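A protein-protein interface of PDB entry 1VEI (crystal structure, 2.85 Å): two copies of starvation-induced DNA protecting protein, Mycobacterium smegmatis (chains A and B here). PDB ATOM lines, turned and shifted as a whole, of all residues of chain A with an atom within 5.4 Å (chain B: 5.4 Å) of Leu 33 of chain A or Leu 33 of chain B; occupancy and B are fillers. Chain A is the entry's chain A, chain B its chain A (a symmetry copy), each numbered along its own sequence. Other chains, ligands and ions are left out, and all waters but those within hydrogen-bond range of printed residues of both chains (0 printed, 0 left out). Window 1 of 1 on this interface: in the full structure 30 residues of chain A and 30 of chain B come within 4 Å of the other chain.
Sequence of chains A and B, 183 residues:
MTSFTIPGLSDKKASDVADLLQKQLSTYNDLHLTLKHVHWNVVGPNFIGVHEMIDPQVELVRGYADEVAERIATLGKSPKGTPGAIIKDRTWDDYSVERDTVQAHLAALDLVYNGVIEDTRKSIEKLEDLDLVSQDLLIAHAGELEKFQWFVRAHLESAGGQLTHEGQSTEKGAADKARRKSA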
ATOM      1  N   TYR A  28      -1.707 -12.565 -19.111  1.00  0.00           N
ATOM      2  CA  TYR A  28      -1.075 -13.617 -19.888  1.00  0.00           C
ATOM      3  C   TYR A  28       0.436 -13.505 -19.816  1.00  0.00           C
ATOM      4  O   TYR A  28       1.112 -14.458 -19.436  1.00  0.00           O
ATOM      5  CB  TYR A  28      -1.522 -13.541 -21.348  1.00  0.00           C
ATOM      6  CG  TYR A  28      -2.959 -13.978 -21.580  1.00  0.00           C
ATOM      7  CD1 TYR A  28      -3.680 -13.520 -22.694  1.00  0.00           C
ATOM      8  CD2 TYR A  28      -3.599 -14.841 -20.688  1.00  0.00           C
ATOM      9  CE1 TYR A  28      -4.997 -13.906 -22.905  1.00  0.00           C
ATOM     10  CE2 TYR A  28      -4.912 -15.236 -20.893  1.00  0.00           C
ATOM     11  CZ  TYR A  28      -5.603 -14.762 -21.997  1.00  0.00           C
ATOM     12  OH  TYR A  28      -6.913 -15.130 -22.185  1.00  0.00           O
ATOM     13  N   ASN A  29       0.972 -12.343 -20.175  1.00  0.00           N
ATOM     14  CA  ASN A  29       2.425 -12.164 -20.153  1.00  0.00           C
ATOM     15  C   ASN A  29       3.047 -12.520 -18.814  1.00  0.00           C
ATOM     16  O   ASN A  29       4.146 -13.071 -18.742  1.00  0.00           O
ATOM     17  CB  ASN A  29       2.800 -10.737 -20.523  1.00  0.00           C
ATOM     18  CG  ASN A  29       2.726 -10.492 -22.001  1.00  0.00           C
ATOM     19  OD1 ASN A  29       3.263 -11.260 -22.803  1.00  0.00           O
ATOM     20  ND2 ASN A  29       2.066  -9.416 -22.379  1.00  0.00           N
ATOM     21  N   ASP A  30       2.333 -12.194 -17.749  1.00  0.00           N
ATOM     22  CA  ASP A  30       2.802 -12.478 -16.411  1.00  0.00           C
ATOM     23  C   ASP A  30       2.786 -13.996 -16.252  1.00  0.00           C
ATOM     24  O   ASP A  30       3.747 -14.600 -15.764  1.00  0.00           O
ATOM     25  CB  ASP A  30       1.862 -11.813 -15.389  1.00  0.00           C
ATOM     26  CG  ASP A  30       2.309 -12.031 -13.962  1.00  0.00           C
ATOM     27  OD1 ASP A  30       3.361 -11.489 -13.580  1.00  0.00           O
ATOM     28  OD2 ASP A  30       1.613 -12.752 -13.223  1.00  0.00           O
ATOM     29  N   LEU A  31       1.686 -14.594 -16.699  1.00  0.00           N
ATOM     30  CA  LEU A  31       1.466 -16.029 -16.611  1.00  0.00           C
ATOM     31  C   LEU A  31       2.413 -16.918 -17.414  1.00  0.00           C
ATOM     32  O   LEU A  31       2.861 -17.954 -16.918  1.00  0.00           O
ATOM     33  CB  LEU A  31       0.032 -16.344 -17.015  1.00  0.00           C
ATOM     34  CG  LEU A  31      -0.373 -17.821 -17.016  1.00  0.00           C
ATOM     35  CD1 LEU A  31      -0.348 -18.389 -15.602  1.00  0.00           C
ATOM     36  CD2 LEU A  31      -1.754 -17.955 -17.622  1.00  0.00           C
ATOM     37  N   HIS A  32       2.718 -16.549 -18.653  1.00  0.00           N
ATOM     38  CA  HIS A  32       3.605 -17.407 -19.409  1.00  0.00           C
ATOM     39  C   HIS A  32       5.047 -17.252 -18.964  1.00  0.00           C
ATOM     40  O   HIS A  32       5.894 -18.059 -19.320  1.00  0.00           O
ATOM     41  CB  HIS A  32       3.405 -17.226 -20.936  1.00  0.00           C
ATOM     42  CG  HIS A  32       3.989 -15.976 -21.524  1.00  0.00           C
ATOM     43  ND1 HIS A  32       5.350 -15.771 -21.649  1.00  0.00           N
ATOM     44  CD2 HIS A  32       3.393 -14.923 -22.138  1.00  0.00           C
ATOM     45  CE1 HIS A  32       5.564 -14.649 -22.318  1.00  0.00           C
ATOM     46  NE2 HIS A  32       4.393 -14.116 -22.627  1.00  0.00           N
ATOM     47  N   LEU A  33       5.320 -16.231 -18.157  1.00  0.00           N
ATOM     48  CA  LEU A  33       6.670 -16.032 -17.623  1.00  0.00           C
ATOM     49  C   LEU A  33       6.745 -16.838 -16.339  1.00  0.00           C
ATOM     50  O   LEU A  33       7.727 -17.528 -16.079  1.00  0.00           O
ATOM     51  CB  LEU A  33       6.948 -14.562 -17.307  1.00  0.00           C
ATOM     52  CG  LEU A  33       7.280 -13.649 -18.489  1.00  0.00           C
ATOM     53  CD1 LEU A  33       7.654 -12.270 -17.996  1.00  0.00           C
ATOM     54  CD2 LEU A  33       8.431 -14.253 -19.276  1.00  0.00           C
ATOM     55  N   THR A  34       5.683 -16.743 -15.549  1.00  0.00           N
ATOM     56  CA  THR A  34       5.561 -17.462 -14.292  1.00  0.00           C
ATOM     57  C   THR A  34       5.634 -18.955 -14.557  1.00  0.00           C
ATOM     58  O   THR A  34       6.466 -19.659 -13.978  1.00  0.00           O
ATOM     59  CB  THR A  34       4.214 -17.176 -13.640  1.00  0.00           C
ATOM     60  OG1 THR A  34       4.085 -15.769 -13.423  1.00  0.00           O
ATOM     61  CG2 THR A  34       4.096 -17.902 -12.334  1.00  0.00           C
ATOM     62  N   LEU A  35       4.730 -19.421 -15.420  1.00  0.00           N
ATOM     63  CA  LEU A  35       4.620 -20.833 -15.834  1.00  0.00           C
ATOM     64  C   LEU A  35       6.013 -21.351 -16.160  1.00  0.00           C
ATOM     65  O   LEU A  35       6.432 -22.411 -15.704  1.00  0.00           O
ATOM     66  CB  LEU A  35       3.746 -20.919 -17.088  1.00  0.00           C
ATOM     67  CG  LEU A  35       2.527 -21.835 -17.181  1.00  0.00           C
ATOM     68  CD1 LEU A  35       2.017 -22.257 -15.796  1.00  0.00           C
ATOM     69  CD2 LEU A  35       1.456 -21.088 -17.980  1.00  0.00           C
ATOM     70  N   LYS A  36       6.727 -20.563 -16.950  1.00  0.00           N
ATOM     71  CA  LYS A  36       8.070 -20.891 -17.362  1.00  0.00           C
ATOM     72  C   LYS A  36       8.996 -20.943 -16.137  1.00  0.00           C
ATOM     73  O   LYS A  36       9.881 -21.802 -16.045  1.00  0.00           O
ATOM     74  CB  LYS A  36       8.535 -19.836 -18.368  1.00  0.00           C
ATOM     75  CG  LYS A  36       9.541 -20.331 -19.389  1.00  0.00           C
ATOM     76  CD  LYS A  36       9.049 -21.590 -20.118  1.00  0.00           C
ATOM     77  CE  LYS A  36      10.040 -22.033 -21.176  1.00  0.00           C
ATOM     78  NZ  LYS A  36       9.773 -23.397 -21.697  1.00  0.00           N
ATOM     79  N   HIS A  37       8.779 -20.024 -15.196  1.00  0.00           N
ATOM     80  CA  HIS A  37       9.573 -19.960 -13.971  1.00  0.00           C
ATOM     81  C   HIS A  37       9.440 -21.240 -13.154  1.00  0.00           C
ATOM     82  O   HIS A  37      10.436 -21.785 -12.682  1.00  0.00           O
ATOM     83  CB  HIS A  37       9.134 -18.764 -13.108  1.00  0.00           C
ATOM     84  CG  HIS A  37       9.771 -18.722 -11.746  1.00  0.00           C
ATOM     85  ND1 HIS A  37      11.076 -18.324 -11.539  1.00  0.00           N
ATOM     86  CD2 HIS A  37       9.285 -19.055 -10.524  1.00  0.00           C
ATOM     87  CE1 HIS A  37      11.365 -18.418 -10.255  1.00  0.00           C
ATOM     88  NE2 HIS A  37      10.296 -18.860  -9.617  1.00  0.00           N
ATOM     89  N   VAL A  38       8.208 -21.719 -12.983  1.00  0.00           N
ATOM     90  CA  VAL A  38       7.992 -22.932 -12.194  1.00  0.00           C
ATOM     91  C   VAL A  38       8.460 -24.158 -12.956  1.00  0.00           C
ATOM     92  O   VAL A  38       8.720 -25.216 -12.373  1.00  0.00           O
ATOM     93  CB  VAL A  38       6.500 -23.109 -11.795  1.00  0.00           C
ATOM     94  CG1 VAL A  38       5.721 -21.832 -12.140  1.00  0.00           C
ATOM     95  CG2 VAL A  38       5.909 -24.346 -12.452  1.00  0.00           C
ATOM     96  N   GLY A  81       3.334  -4.187 -24.102  1.00  0.00           N
ATOM     97  CA  GLY A  81       3.930  -5.437 -23.680  1.00  0.00           C
ATOM     98  C   GLY A  81       5.313  -5.439 -23.067  1.00  0.00           C
ATOM     99  O   GLY A  81       5.956  -6.482 -23.017  1.00  0.00           O
ATOM    100  N   THR A  82       5.796  -4.297 -22.606  1.00  0.00           N
ATOM    101  CA  THR A  82       7.111  -4.258 -21.973  1.00  0.00           C
ATOM    102  C   THR A  82       6.933  -4.636 -20.500  1.00  0.00           C
ATOM    103  O   THR A  82       5.833  -4.514 -19.959  1.00  0.00           O
ATOM    104  CB  THR A  82       7.725  -2.866 -22.090  1.00  0.00           C
ATOM    105  OG1 THR A  82       6.676  -1.892 -22.054  1.00  0.00           O
ATOM    106  CG2 THR A  82       8.499  -2.734 -23.388  1.00  0.00           C
ATOM    107  N   PRO A  83       8.006  -5.110 -19.836  1.00  0.00           N
ATOM    108  CA  PRO A  83       7.960  -5.513 -18.418  1.00  0.00           C
ATOM    109  C   PRO A  83       7.287  -4.502 -17.486  1.00  0.00           C
ATOM    110  O   PRO A  83       6.659  -4.877 -16.492  1.00  0.00           O
ATOM    111  CB  PRO A  83       9.427  -5.727 -18.071  1.00  0.00           C
ATOM    112  CG  PRO A  83      10.017  -6.183 -19.385  1.00  0.00           C
ATOM    113  CD  PRO A  83       9.375  -5.233 -20.374  1.00  0.00           C
ATOM    114  N   ILE A  86       3.502  -4.506 -17.598  1.00  0.00           N
ATOM    115  CA  ILE A  86       2.986  -5.687 -16.921  1.00  0.00           C
ATOM    116  C   ILE A  86       2.775  -5.313 -15.477  1.00  0.00           C
ATOM    117  O   ILE A  86       1.650  -5.317 -14.995  1.00  0.00           O
ATOM    118  CB  ILE A  86       3.978  -6.879 -16.987  1.00  0.00           C
ATOM    119  CG1 ILE A  86       4.235  -7.270 -18.441  1.00  0.00           C
ATOM    120  CG2 ILE A  86       3.419  -8.089 -16.232  1.00  0.00           C
ATOM    121  CD1 ILE A  86       5.320  -8.321 -18.574  1.00  0.00           C
ATOM    122  N   TYR B  28      17.318 -11.386 -21.733  1.00  0.00           N
ATOM    123  CA  TYR B  28      16.547 -12.088 -22.745  1.00  0.00           C
ATOM    124  C   TYR B  28      15.059 -11.904 -22.514  1.00  0.00           C
ATOM    125  O   TYR B  28      14.345 -11.452 -23.405  1.00  0.00           O
ATOM    126  CB  TYR B  28      16.883 -13.581 -22.726  1.00  0.00           C
ATOM    127  CG  TYR B  28      18.260 -13.913 -23.278  1.00  0.00           C
ATOM    128  CD1 TYR B  28      18.924 -15.088 -22.896  1.00  0.00           C
ATOM    129  CD2 TYR B  28      18.900 -13.053 -24.176  1.00  0.00           C
ATOM    130  CE1 TYR B  28      20.187 -15.392 -23.387  1.00  0.00           C
ATOM    131  CE2 TYR B  28      20.159 -13.349 -24.675  1.00  0.00           C
ATOM    132  CZ  TYR B  28      20.796 -14.514 -24.274  1.00  0.00           C
ATOM    133  OH  TYR B  28      22.054 -14.795 -24.746  1.00  0.00           O
ATOM    134  N   ASN B  29      14.589 -12.245 -21.319  1.00  0.00           N
ATOM    135  CA  ASN B  29      13.161 -12.116 -21.027  1.00  0.00           C
ATOM    136  C   ASN B  29      12.618 -10.726 -21.312  1.00  0.00           C
ATOM    137  O   ASN B  29      11.489 -10.557 -21.775  1.00  0.00           O
ATOM    138  CB  ASN B  29      12.867 -12.487 -19.581  1.00  0.00           C
ATOM    139  CG  ASN B  29      12.845 -13.971 -19.366  1.00  0.00           C
ATOM    140  OD1 ASN B  29      12.187 -14.713 -20.101  1.00  0.00           O
ATOM    141  ND2 ASN B  29      13.553 -14.423 -18.350  1.00  0.00           N
ATOM    142  N   ASP B  30      13.437  -9.725 -21.026  1.00  0.00           N
ATOM    143  CA  ASP B  30      13.054  -8.350 -21.252  1.00  0.00           C
ATOM    144  C   ASP B  30      12.966  -8.160 -22.763  1.00  0.00           C
ATOM    145  O   ASP B  30      12.002  -7.586 -23.283  1.00  0.00           O
ATOM    146  CB  ASP B  30      14.119  -7.417 -20.647  1.00  0.00           C
ATOM    147  CG  ASP B  30      13.770  -5.957 -20.806  1.00  0.00           C
ATOM    148  OD1 ASP B  30      12.795  -5.508 -20.177  1.00  0.00           O
ATOM    149  OD2 ASP B  30      14.464  -5.258 -21.568  1.00  0.00           O
ATOM    150  N   LEU B  31      13.979  -8.677 -23.452  1.00  0.00           N
ATOM    151  CA  LEU B  31      14.093  -8.576 -24.898  1.00  0.00           C
ATOM    152  C   LEU B  31      13.022  -9.283 -25.723  1.00  0.00           C
ATOM    153  O   LEU B  31      12.536  -8.732 -26.714  1.00  0.00           O
ATOM    154  CB  LEU B  31      15.463  -9.081 -25.331  1.00  0.00           C
ATOM    155  CG  LEU B  31      15.751  -9.081 -26.835  1.00  0.00           C
ATOM    156  CD1 LEU B  31      15.794  -7.656 -27.378  1.00  0.00           C
ATOM    157  CD2 LEU B  31      17.068  -9.788 -27.086  1.00  0.00           C
ATOM    158  N   HIS B  32      12.649 -10.503 -25.351  1.00  0.00           N
ATOM    159  CA  HIS B  32      11.642 -11.171 -26.149  1.00  0.00           C
ATOM    160  C   HIS B  32      10.255 -10.619 -25.874  1.00  0.00           C
ATOM    161  O   HIS B  32       9.324 -10.891 -26.618  1.00  0.00           O
ATOM    162  CB  HIS B  32      11.735 -12.711 -26.008  1.00  0.00           C
ATOM    163  CG  HIS B  32      11.205 -13.280 -24.725  1.00  0.00           C
ATOM    164  ND1 HIS B  32       9.858 -13.304 -24.417  1.00  0.00           N
ATOM    165  CD2 HIS B  32      11.830 -13.961 -23.732  1.00  0.00           C
ATOM    166  CE1 HIS B  32       9.680 -13.978 -23.293  1.00  0.00           C
ATOM    167  NE2 HIS B  32      10.861 -14.389 -22.857  1.00  0.00           N
ATOM    168  N   LEU B  33      10.125  -9.815 -24.824  1.00  0.00           N
ATOM    169  CA  LEU B  33       8.841  -9.183 -24.512  1.00  0.00           C
ATOM    170  C   LEU B  33       8.805  -7.882 -25.288  1.00  0.00           C
ATOM    171  O   LEU B  33       7.797  -7.531 -25.895  1.00  0.00           O
ATOM    172  CB  LEU B  33       8.702  -8.879 -23.018  1.00  0.00           C
ATOM    173  CG  LEU B  33       8.351 -10.052 -22.101  1.00  0.00           C
ATOM    174  CD1 LEU B  33       8.123  -9.562 -20.690  1.00  0.00           C
ATOM    175  CD2 LEU B  33       7.098 -10.735 -22.626  1.00  0.00           C
ATOM    176  N   THR B  34       9.930  -7.177 -25.264  1.00  0.00           N
ATOM    177  CA  THR B  34      10.094  -5.917 -25.971  1.00  0.00           C
ATOM    178  C   THR B  34       9.886  -6.143 -27.458  1.00  0.00           C
ATOM    179  O   THR B  34       9.051  -5.488 -28.085  1.00  0.00           O
ATOM    180  CB  THR B  34      11.507  -5.377 -25.780  1.00  0.00           C
ATOM    181  OG1 THR B  34      11.759  -5.202 -24.385  1.00  0.00           O
ATOM    182  CG2 THR B  34      11.669  -4.069 -26.492  1.00  0.00           C
ATOM    183  N   LEU B  35      10.682  -7.064 -28.006  1.00  0.00           N
ATOM    184  CA  LEU B  35      10.651  -7.454 -29.429  1.00  0.00           C
ATOM    185  C   LEU B  35       9.200  -7.661 -29.840  1.00  0.00           C
ATOM    186  O   LEU B  35       8.739  -7.151 -30.858  1.00  0.00           O
ATOM    187  CB  LEU B  35      11.414  -8.769 -29.602  1.00  0.00           C
ATOM    188  CG  LEU B  35      12.547  -8.936 -30.612  1.00  0.00           C
ATOM    189  CD1 LEU B  35      13.131  -7.584 -31.052  1.00  0.00           C
ATOM    190  CD2 LEU B  35      13.608  -9.831 -29.964  1.00  0.00           C
ATOM    191  N   LYS B  36       8.490  -8.410 -29.012  1.00  0.00           N
ATOM    192  CA  LYS B  36       7.098  -8.711 -29.240  1.00  0.00           C
ATOM    193  C   LYS B  36       6.267  -7.417 -29.201  1.00  0.00           C
ATOM    194  O   LYS B  36       5.331  -7.240 -29.986  1.00  0.00           O
ATOM    195  CB  LYS B  36       6.637  -9.701 -28.169  1.00  0.00           C
ATOM    196  CG  LYS B  36       5.519 -10.630 -28.600  1.00  0.00           C
ATOM    197  CD  LYS B  36       5.854 -11.368 -29.905  1.00  0.00           C
ATOM    198  CE  LYS B  36       4.752 -12.337 -30.285  1.00  0.00           C
ATOM    199  NZ  LYS B  36       4.874 -12.847 -31.673  1.00  0.00           N
ATOM    200  N   HIS B  37       6.628  -6.516 -28.286  1.00  0.00           N
ATOM    201  CA  HIS B  37       5.939  -5.236 -28.141  1.00  0.00           C
ATOM    202  C   HIS B  37       6.038  -4.404 -29.415  1.00  0.00           C
ATOM    203  O   HIS B  37       5.043  -3.845 -29.873  1.00  0.00           O
ATOM    204  CB  HIS B  37       6.536  -4.435 -26.970  1.00  0.00           C
ATOM    205  CG  HIS B  37       6.012  -3.029 -26.858  1.00  0.00           C
ATOM    206  ND1 HIS B  37       4.761  -2.732 -26.355  1.00  0.00           N
ATOM    207  CD2 HIS B  37       6.566  -1.842 -27.208  1.00  0.00           C
ATOM    208  CE1 HIS B  37       4.567  -1.427 -26.406  1.00  0.00           C
ATOM    209  NE2 HIS B  37       5.646  -0.864 -26.919  1.00  0.00           N
ATOM    210  N   VAL B  38       7.238  -4.316 -29.987  1.00  0.00           N
ATOM    211  CA  VAL B  38       7.422  -3.521 -31.199  1.00  0.00           C
ATOM    212  C   VAL B  38       6.803  -4.219 -32.396  1.00  0.00           C
ATOM    213  O   VAL B  38       6.509  -3.594 -33.422  1.00  0.00           O
ATOM    214  CB  VAL B  38       8.923  -3.233 -31.487  1.00  0.00           C
ATOM    215  CG1 VAL B  38       9.767  -3.665 -30.280  1.00  0.00           C
ATOM    216  CG2 VAL B  38       9.363  -3.907 -32.776  1.00  0.00           C
ATOM    217  N   GLY B  81      12.560 -16.156 -13.066  1.00  0.00           N
ATOM    218  CA  GLY B  81      11.905 -15.663 -14.259  1.00  0.00           C
ATOM    219  C   GLY B  81      10.577 -14.946 -14.143  1.00  0.00           C
ATOM    220  O   GLY B  81       9.863 -14.824 -15.131  1.00  0.00           O
ATOM    221  N   THR B  82      10.221 -14.474 -12.960  1.00  0.00           N
ATOM    222  CA  THR B  82       8.967 -13.742 -12.808  1.00  0.00           C
ATOM    223  C   THR B  82       9.231 -12.280 -13.176  1.00  0.00           C
ATOM    224  O   THR B  82      10.375 -11.827 -13.131  1.00  0.00           O
ATOM    225  CB  THR B  82       8.455 -13.843 -11.375  1.00  0.00           C
ATOM    226  OG1 THR B  82       9.574 -13.907 -10.485  1.00  0.00           O
ATOM    227  CG2 THR B  82       7.593 -15.079 -11.202  1.00  0.00           C
ATOM    228  N   PRO B  83       8.179 -11.524 -13.554  1.00  0.00           N
ATOM    229  CA  PRO B  83       8.304 -10.107 -13.936  1.00  0.00           C
ATOM    230  C   PRO B  83       9.125  -9.251 -12.967  1.00  0.00           C
ATOM    231  O   PRO B  83       9.797  -8.301 -13.373  1.00  0.00           O
ATOM    232  CB  PRO B  83       6.857  -9.642 -14.031  1.00  0.00           C
ATOM    233  CG  PRO B  83       6.132 -10.898 -14.459  1.00  0.00           C
ATOM    234  CD  PRO B  83       6.766 -11.953 -13.577  1.00  0.00           C
ATOM    235  N   ILE B  86      12.877  -9.653 -13.269  1.00  0.00           N
ATOM    236  CA  ILE B  86      13.352  -8.992 -14.476  1.00  0.00           C
ATOM    237  C   ILE B  86      13.704  -7.576 -14.098  1.00  0.00           C
ATOM    238  O   ILE B  86      14.859  -7.182 -14.182  1.00  0.00           O
ATOM    239  CB  ILE B  86      12.270  -8.955 -15.588  1.00  0.00           C
ATOM    240  CG1 ILE B  86      11.870 -10.377 -15.981  1.00  0.00           C
ATOM    241  CG2 ILE B  86      12.791  -8.220 -16.826  1.00  0.00           C
ATOM    242  CD1 ILE B  86      10.700 -10.403 -16.945  1.00  0.00           C
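The backbone NH of Gly 81 of chain B is in hydrogen-bond range of a ring nitrogen (ND1) of His 37 of chain A (3.0 Å). N of Gly 81 of chain A sits at hydrogen-bond distance from ND1 of His 37 of chain B.
Of the 15 printed residues of chain A, 7 touch a printed residue of chain B. Printed residues of chain A that touch a printed residue of chain B: Asn 29, Asp 30, Leu 33, His 37, Gly 81, Pro 83 and Ile 86. Of the 15 printed residues of chain B, 7 touch a printed residue of chain A. Along chain B the printed residues that touch a printed residue of chain A span positions 29 to 86. Among the printed residues, 11 pairs touch across the chains.
Asn 29 of chain A touches Leu 33 of chain B, and with the chains exchanged Leu 33 of chain A touches Asn 29 of chain B. Asp 30 of chain A touches Pro 83 of chain B, and with the chains exchanged Pro 83 of chain A touches Asp 30 of chain B. Leu 33 of chain A touches Gly 81 of chain B, and with the chains exchanged Gly 81 of chain A touches Leu 33 of chain B. Leu 33 of chain A touches Ile 86 of chain B, and with the chains exchanged Ile 86 of chain A touches Leu 33 of chain B. 15 positions are printed for both chains.
Among the printed residues, merely in contact across the chains: Pro 83 of chain A with Asp 30 of chain B (3.0 Å), Asp 30 of chain A with Pro 83 of chain B (3.0 Å), Gly 81 of chain A with Leu 33 of chain B (3.6 Å), Leu 33 of chain A with Gly 81 of chain B (3.6 Å), Leu 33 of chain A with Ile 86 of chain B (3.7 Å), Ile 86 of chain A with Leu 33 of chain B (3.7 Å), Leu 33 of chain A with Leu 33 of chain B (3.8 Å), Leu 33 of chain A with Asn 29 of chain B (3.9 Å) and Asn 29 of chain A with Leu 33 of chain B (3.9 Å).
O of Asp 30 of chain B is in hydrogen-bond range of OG1 of Thr 34 of chain B (2.6 Å). The side-chain amide oxygen of Asn 29 of chain A sits at hydrogen-bond distance from a ring nitrogen (NE2) of His 32 of chain A, at 3.1 Å. O of Asp 30 of chain A sits at hydrogen-bond distance from OG1 of Thr 34 of chain A, at 2.6 Å. A ring nitrogen (NE2) of His 32 of chain B sits at hydrogen-bond distance from the side-chain amide oxygen (OD1) of Asn 29 of chain B (3.1 Å).
Of chain B, only Asn 29, Leu 33, Gly 81 and Ile 86 come within 4 Å of Leu 33 of chain A. Leu 33 of chain B touches just these residues of chain A: Asn 29, Leu 33, Gly 81 and Ile 86. Printed residues of chain A within 4 Å of His 37 of chain B: Gly 81 (3.0 Å). Of the printed residues of chain A, Gly 81 of chain B touches Leu 33 and His 37. Of the printed residues of chain A, Pro 83 of chain B touches Asp 30. Printed residues of chain B within 4 Å of His 37 of chain A: Gly 81 (3.0 Å). Printed residues of chain B within 4 Å of Asn 29 of chain A: Leu 33. Lys 36 of chain A touches none of the printed residues of chain B. Leu 31 of chain A touches none of the printed residues of chain B. The nearest residue of chain B that does not touch Leu 33 of chain A is Pro 83 of chain B (4.1 Å). The nearest printed residue of chain B that does not touch Asp 30 of chain A is Thr 82 of chain B (5.9 Å).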
